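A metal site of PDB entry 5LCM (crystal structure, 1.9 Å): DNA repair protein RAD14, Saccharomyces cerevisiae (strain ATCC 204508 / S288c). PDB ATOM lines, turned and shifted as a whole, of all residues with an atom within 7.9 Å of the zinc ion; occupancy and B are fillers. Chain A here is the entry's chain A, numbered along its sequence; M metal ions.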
ATOM      1  N   LYS A   3      -8.379  -9.741  -9.065  1.00  0.00           N
ATOM      2  CA  LYS A   3      -7.753  -9.777 -10.401  1.00  0.00           C
ATOM      3  C   LYS A   3      -8.719 -10.267 -11.461  1.00  0.00           C
ATOM      4  O   LYS A   3      -9.621 -11.068 -11.176  1.00  0.00           O
ATOM      5  CB  LYS A   3      -6.558 -10.703 -10.409  1.00  0.00           C
ATOM      6  CG  LYS A   3      -5.569 -10.423  -9.307  1.00  0.00           C
ATOM      7  CD  LYS A   3      -4.835  -9.137  -9.527  1.00  0.00           C
ATOM      8  CE  LYS A   3      -4.168  -8.636  -8.222  1.00  0.00           C
ATOM      9  NZ  LYS A   3      -2.707  -8.846  -8.285  1.00  0.00           N
ATOM     10  N   CYS A   4      -8.480  -9.858 -12.684  1.00  0.00           N
ATOM     11  CA  CYS A   4      -9.271 -10.315 -13.777  1.00  0.00           C
ATOM     12  C   CYS A   4      -9.173 -11.855 -13.887  1.00  0.00           C
ATOM     13  O   CYS A   4      -8.087 -12.448 -13.705  1.00  0.00           O
ATOM     14  CB  CYS A   4      -8.811  -9.619 -15.045  1.00  0.00           C
ATOM     15  SG  CYS A   4      -9.341 -10.426 -16.558  1.00  0.00           S
ATOM     16  N   ILE A   5     -10.297 -12.515 -14.089  1.00  0.00           N
ATOM     17  CA  ILE A   5     -10.343 -13.998 -14.125  1.00  0.00           C
ATOM     18  C   ILE A   5      -9.679 -14.625 -15.369  1.00  0.00           C
ATOM     19  O   ILE A   5      -9.364 -15.776 -15.323  1.00  0.00           O
ATOM     20  CB  ILE A   5     -11.787 -14.543 -13.977  1.00  0.00           C
ATOM     21  CG1 ILE A   5     -12.626 -14.096 -15.149  1.00  0.00           C
ATOM     22  CG2 ILE A   5     -12.400 -14.042 -12.675  1.00  0.00           C
ATOM     23  CD1 ILE A   5     -13.997 -14.715 -15.235  1.00  0.00           C
ATOM     24  N   GLU A   6      -9.389 -13.876 -16.444  1.00  0.00           N
ATOM     25  CA  GLU A   6      -8.622 -14.440 -17.587  1.00  0.00           C
ATOM     26  C   GLU A   6      -7.145 -14.202 -17.445  1.00  0.00           C
ATOM     27  O   GLU A   6      -6.356 -15.101 -17.480  1.00  0.00           O
ATOM     28  CB  GLU A   6      -9.083 -13.831 -18.929  1.00  0.00           C
ATOM     29  CG  GLU A   6     -10.540 -14.146 -19.262  1.00  0.00           C
ATOM     30  CD  GLU A   6     -10.746 -15.600 -19.656  1.00  0.00           C
ATOM     31  OE1 GLU A   6     -11.909 -16.125 -19.552  1.00  0.00           O
ATOM     32  OE2 GLU A   6      -9.759 -16.219 -20.037  1.00  0.00           O
ATOM     33  N   CYS A   7      -6.744 -12.958 -17.306  1.00  0.00           N
ATOM     34  CA  CYS A   7      -5.332 -12.621 -17.273  1.00  0.00           C
ATOM     35  C   CYS A   7      -4.697 -12.759 -15.898  1.00  0.00           C
ATOM     36  O   CYS A   7      -3.498 -12.899 -15.806  1.00  0.00           O
ATOM     37  CB  CYS A   7      -5.072 -11.243 -17.891  1.00  0.00           C
ATOM     38  SG  CYS A   7      -5.628  -9.814 -16.970  1.00  0.00           S
ATOM     39  N   HIS A   8      -5.497 -12.728 -14.831  1.00  0.00           N
ATOM     40  CA  HIS A   8      -4.973 -12.665 -13.458  1.00  0.00           C
ATOM     41  C   HIS A   8      -3.979 -11.552 -13.144  1.00  0.00           C
ATOM     42  O   HIS A   8      -3.271 -11.650 -12.203  1.00  0.00           O
ATOM     43  CB  HIS A   8      -4.365 -14.016 -13.018  1.00  0.00           C
ATOM     44  CG  HIS A   8      -5.305 -15.148 -13.224  1.00  0.00           C
ATOM     45  ND1 HIS A   8      -6.473 -15.289 -12.493  1.00  0.00           N
ATOM     46  CD2 HIS A   8      -5.330 -16.122 -14.178  1.00  0.00           C
ATOM     47  CE1 HIS A   8      -7.139 -16.349 -12.938  1.00  0.00           C
ATOM     48  NE2 HIS A   8      -6.484 -16.840 -13.983  1.00  0.00           N
ATOM     49  N   ILE A   9      -4.060 -10.440 -13.887  1.00  0.00           N
ATOM     50  CA  ILE A   9      -3.127  -9.336 -13.750  1.00  0.00           C
ATOM     51  C   ILE A   9      -3.836  -8.008 -13.517  1.00  0.00           C
ATOM     52  O   ILE A   9      -3.586  -7.393 -12.554  1.00  0.00           O
ATOM     53  CB  ILE A   9      -2.253  -9.244 -15.019  1.00  0.00           C
ATOM     54  CG1 ILE A   9      -1.355 -10.532 -15.073  1.00  0.00           C
ATOM     55  CG2 ILE A   9      -1.400  -7.940 -14.992  1.00  0.00           C
ATOM     56  CD1 ILE A   9      -0.602 -10.588 -16.368  1.00  0.00           C
ATOM     57  N   ASN A  10      -4.708  -7.622 -14.436  1.00  0.00           N
ATOM     58  CA  ASN A  10      -5.503  -6.401 -14.331  1.00  0.00           C
ATOM     59  C   ASN A  10      -6.464  -6.370 -13.092  1.00  0.00           C
ATOM     60  O   ASN A  10      -7.057  -7.398 -12.691  1.00  0.00           O
ATOM     61  CB  ASN A  10      -6.264  -6.147 -15.644  1.00  0.00           C
ATOM     62  CG  ASN A  10      -5.417  -5.333 -16.656  1.00  0.00           C
ATOM     63  OD1 ASN A  10      -4.610  -4.473 -16.260  1.00  0.00           O
ATOM     64  ND2 ASN A  10      -5.643  -5.577 -17.958  1.00  0.00           N
ATOM     65  N   ILE A  11      -6.605  -5.187 -12.522  1.00  0.00           N
ATOM     66  CA  ILE A  11      -7.536  -4.963 -11.444  1.00  0.00           C
ATOM     67  C   ILE A  11      -8.684  -4.014 -11.849  1.00  0.00           C
ATOM     68  O   ILE A  11      -9.587  -3.801 -11.032  1.00  0.00           O
ATOM     69  CB  ILE A  11      -6.792  -4.495 -10.163  1.00  0.00           C
ATOM     70  CG1 ILE A  11      -6.061  -3.124 -10.314  1.00  0.00           C
ATOM     71  CG2 ILE A  11      -5.788  -5.577  -9.652  1.00  0.00           C
ATOM     72  CD1 ILE A  11      -5.508  -2.581  -8.968  1.00  0.00           C
ATOM     73  N   GLU A  12      -8.666  -3.448 -13.047  1.00  0.00           N
ATOM     74  CA  GLU A  12      -9.745  -2.545 -13.502  1.00  0.00           C
ATOM     75  C   GLU A  12     -10.544  -3.373 -14.501  1.00  0.00           C
ATOM     76  O   GLU A  12     -10.019  -3.765 -15.551  1.00  0.00           O
ATOM     77  CB  GLU A  12      -9.229  -1.278 -14.215  1.00  0.00           C
ATOM     78  CG  GLU A  12      -8.229  -0.449 -13.459  1.00  0.00           C
ATOM     79  CD  GLU A  12      -8.849   0.205 -12.271  1.00  0.00           C
ATOM     80  OE1 GLU A  12     -10.086   0.409 -12.342  1.00  0.00           O
ATOM     81  OE2 GLU A  12      -8.143   0.507 -11.276  1.00  0.00           O
ATOM     82  N   MET A  13     -11.778  -3.683 -14.165  1.00  0.00           N
ATOM     83  CA  MET A  13     -12.585  -4.537 -14.908  1.00  0.00           C
ATOM     84  C   MET A  13     -13.354  -3.752 -15.955  1.00  0.00           C
ATOM     85  O   MET A  13     -13.544  -2.506 -15.836  1.00  0.00           O
ATOM     86  CB  MET A  13     -13.520  -5.359 -13.976  1.00  0.00           C
ATOM     87  CG  MET A  13     -12.878  -6.074 -12.738  1.00  0.00           C
ATOM     88  SD  MET A  13     -11.694  -7.208 -13.468  1.00  0.00           S
ATOM     89  CE  MET A  13     -10.753  -7.464 -11.971  1.00  0.00           C
ATOM     90  N   GLN A  24     -15.839 -10.575 -13.714  1.00  0.00           N
ATOM     91  CA  GLN A  24     -14.632  -9.946 -13.229  1.00  0.00           C
ATOM     92  C   GLN A  24     -13.580 -10.113 -14.318  1.00  0.00           C
ATOM     93  O   GLN A  24     -12.600 -10.918 -14.181  1.00  0.00           O
ATOM     94  CB  GLN A  24     -14.166 -10.665 -11.989  1.00  0.00           C
ATOM     95  CG  GLN A  24     -15.094 -10.455 -10.846  1.00  0.00           C
ATOM     96  CD  GLN A  24     -14.504  -9.440  -9.936  1.00  0.00           C
ATOM     97  OE1 GLN A  24     -13.780  -9.815  -8.981  1.00  0.00           O
ATOM     98  NE2 GLN A  24     -14.713  -8.149 -10.277  1.00  0.00           N
ATOM     99  N   VAL A  25     -13.775  -9.319 -15.376  1.00  0.00           N
ATOM    100  CA  VAL A  25     -12.993  -9.403 -16.627  1.00  0.00           C
ATOM    101  C   VAL A  25     -12.648  -8.039 -17.156  1.00  0.00           C
ATOM    102  O   VAL A  25     -13.474  -7.139 -17.170  1.00  0.00           O
ATOM    103  CB  VAL A  25     -13.746 -10.117 -17.741  1.00  0.00           C
ATOM    104  CG1 VAL A  25     -12.808 -10.465 -18.909  1.00  0.00           C
ATOM    105  CG2 VAL A  25     -14.329 -11.357 -17.152  1.00  0.00           C
ATOM    106  N   CYS A  26     -11.361  -7.829 -17.410  1.00  0.00           N
ATOM    107  CA  CYS A  26     -10.874  -6.599 -17.942  1.00  0.00           C
ATOM    108  C   CYS A  26     -11.265  -6.499 -19.391  1.00  0.00           C
ATOM    109  O   CYS A  26     -11.583  -7.480 -20.077  1.00  0.00           O
ATOM    110  CB  CYS A  26      -9.335  -6.400 -17.766  1.00  0.00           C
ATOM    111  SG  CYS A  26      -8.288  -7.399 -18.827  1.00  0.00           S
ATOM    112  N   LYS A  27     -11.251  -5.251 -19.848  1.00  0.00           N
ATOM    113  CA  LYS A  27     -11.590  -4.868 -21.184  1.00  0.00           C
ATOM    114  C   LYS A  27     -10.691  -5.577 -22.204  1.00  0.00           C
ATOM    115  O   LYS A  27     -11.164  -6.107 -23.212  1.00  0.00           O
ATOM    116  CB  LYS A  27     -11.617  -3.333 -21.229  1.00  0.00           C
ATOM    117  CG  LYS A  27     -11.542  -2.670 -22.583  1.00  0.00           C
ATOM    118  CD  LYS A  27     -12.810  -2.736 -23.246  1.00  0.00           C
ATOM    119  CE  LYS A  27     -13.656  -1.472 -22.998  1.00  0.00           C
ATOM    120  NZ  LYS A  27     -14.984  -1.760 -23.688  1.00  0.00           N
ATOM    121  N   GLN A  28      -9.380  -5.659 -21.954  1.00  0.00           N
ATOM    122  CA  GLN A  28      -8.467  -6.223 -22.971  1.00  0.00           C
ATOM    123  C   GLN A  28      -8.715  -7.720 -23.125  1.00  0.00           C
ATOM    124  O   GLN A  28      -8.809  -8.251 -24.246  1.00  0.00           O
ATOM    125  CB  GLN A  28      -7.009  -5.936 -22.552  1.00  0.00           C
ATOM    126  CG  GLN A  28      -5.948  -6.662 -23.386  1.00  0.00           C
ATOM    127  CD  GLN A  28      -4.560  -6.233 -23.076  1.00  0.00           C
ATOM    128  OE1 GLN A  28      -4.331  -5.543 -22.128  1.00  0.00           O
ATOM    129  NE2 GLN A  28      -3.660  -6.526 -23.975  1.00  0.00           N
ATOM    130  N   CYS A  29      -8.931  -8.377 -21.993  1.00  0.00           N
ATOM    131  CA  CYS A  29      -9.289  -9.789 -22.014  1.00  0.00           C
ATOM    132  C   CYS A  29     -10.669  -9.993 -22.656  1.00  0.00           C
ATOM    133  O   CYS A  29     -10.866 -10.934 -23.430  1.00  0.00           O
ATOM    134  CB  CYS A  29      -9.223 -10.452 -20.634  1.00  0.00           C
ATOM    135  SG  CYS A  29      -7.590 -10.689 -20.052  1.00  0.00           S
ATOM    136  N   SER A  30     -11.586  -9.100 -22.479  1.00  0.00           N
ATOM    137  CA  SER A  30     -12.891  -9.286 -23.176  1.00  0.00           C
ATOM    138  C   SER A  30     -12.709  -9.320 -24.729  1.00  0.00           C
ATOM    139  O   SER A  30     -13.243 -10.184 -25.413  1.00  0.00           O
ATOM    140  CB  SER A  30     -13.866  -8.189 -22.839  1.00  0.00           C
ATOM    141  OG  SER A  30     -13.420  -6.977 -23.432  1.00  0.00           O
ATOM    142  N   GLU A  32      -9.933 -10.006 -26.353  1.00  0.00           N
ATOM    143  CA  GLU A  32      -9.136 -11.170 -26.692  1.00  0.00           C
ATOM    144  C   GLU A  32      -9.899 -12.494 -26.617  1.00  0.00           C
ATOM    145  O   GLU A  32      -9.438 -13.506 -27.143  1.00  0.00           O
ATOM    146  CB  GLU A  32      -7.862 -11.196 -25.793  1.00  0.00           C
ATOM    147  CG  GLU A  32      -6.953  -9.981 -26.062  1.00  0.00           C
ATOM    148  CD  GLU A  32      -5.764  -9.841 -25.091  1.00  0.00           C
ATOM    149  OE1 GLU A  32      -5.809 -10.444 -23.982  1.00  0.00           O
ATOM    150  OE2 GLU A  32      -4.799  -9.073 -25.427  1.00  0.00           O
ATOM    151  N   HIS A  33     -11.059 -12.526 -25.964  1.00  0.00           N
ATOM    152  CA  HIS A  33     -11.810 -13.763 -25.912  1.00  0.00           C
ATOM    153  C   HIS A  33     -13.283 -13.566 -26.300  1.00  0.00           C
ATOM    154  O   HIS A  33     -14.152 -13.800 -25.460  1.00  0.00           O
ATOM    155  CB  HIS A  33     -11.681 -14.357 -24.503  1.00  0.00           C
ATOM    156  CG  HIS A  33     -10.297 -14.786 -24.198  1.00  0.00           C
ATOM    157  ND1 HIS A  33      -9.732 -15.867 -24.825  1.00  0.00           N
ATOM    158  CD2 HIS A  33      -9.310 -14.241 -23.451  1.00  0.00           C
ATOM    159  CE1 HIS A  33      -8.460 -15.990 -24.463  1.00  0.00           C
ATOM    160  NE2 HIS A  33      -8.213 -15.045 -23.580  1.00  0.00           N
ATOM    161  N   TYR A  37     -17.014 -13.476 -24.359  1.00  0.00           N
ATOM    162  CA  TYR A  37     -17.388 -12.177 -23.803  1.00  0.00           C
ATOM    163  C   TYR A  37     -18.040 -11.277 -24.818  1.00  0.00           C
ATOM    164  O   TYR A  37     -18.370 -10.182 -24.450  1.00  0.00           O
ATOM    165  CB  TYR A  37     -16.163 -11.449 -23.143  1.00  0.00           C
ATOM    166  CG  TYR A  37     -15.502 -12.272 -22.098  1.00  0.00           C
ATOM    167  CD1 TYR A  37     -16.208 -12.713 -20.985  1.00  0.00           C
ATOM    168  CD2 TYR A  37     -14.192 -12.668 -22.213  1.00  0.00           C
ATOM    169  CE1 TYR A  37     -15.647 -13.504 -20.035  1.00  0.00           C
ATOM    170  CE2 TYR A  37     -13.592 -13.433 -21.245  1.00  0.00           C
ATOM    171  CZ  TYR A  37     -14.316 -13.862 -20.161  1.00  0.00           C
ATOM    172  OH  TYR A  37     -13.767 -14.646 -19.172  1.00  0.00           O
HETATM  173 ZN    ZN M   1      -7.715  -9.541 -18.033  1.00  0.00          ZN
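ND2 of Asn 10 lies close to SG of Cys 26 (3.3 Å).
N of Gln 28 lies close to SG of Cys 26 (3.7 Å).
The side-chain sulfur (SG) of Cys 7 lies close to the backbone NH (N) of Asn 10.
The side-chain sulfur (SG) of Cys 7 lies close to the backbone NH (N) of Ile 9.
The backbone NH of Cys 4 is in hydrogen-bond range of the backbone carbonyl oxygen of Asn 10 (2.8 Å).
N of Glu 6 lies close to SG of Cys 4 (3.5 Å).
The backbone carbonyl oxygen (O) of Cys 4 sits close to a ring nitrogen (ND1) of His 8 (3.5 Å).
Within 4 Å of the zinc ion: Cys 4, Cys 7, Cys 26 and Cys 29.
Along chain A the residues within 4 Å of the zinc ion span positions 4 to 29.
The nearest printed residue that does not touch the zinc ion is Asn 10 (4.4 Å).
SG of Cys 29 binds the zinc ion (2.3 Å).
The side-chain sulfur (SG) of Cys 26 is bound to the zinc ion, at 2.4 Å.
The zinc ion is bound by SG of Cys 7 (2.4 Å).
The zinc ion is bound by SG of Cys 4, 2.4 Å away.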
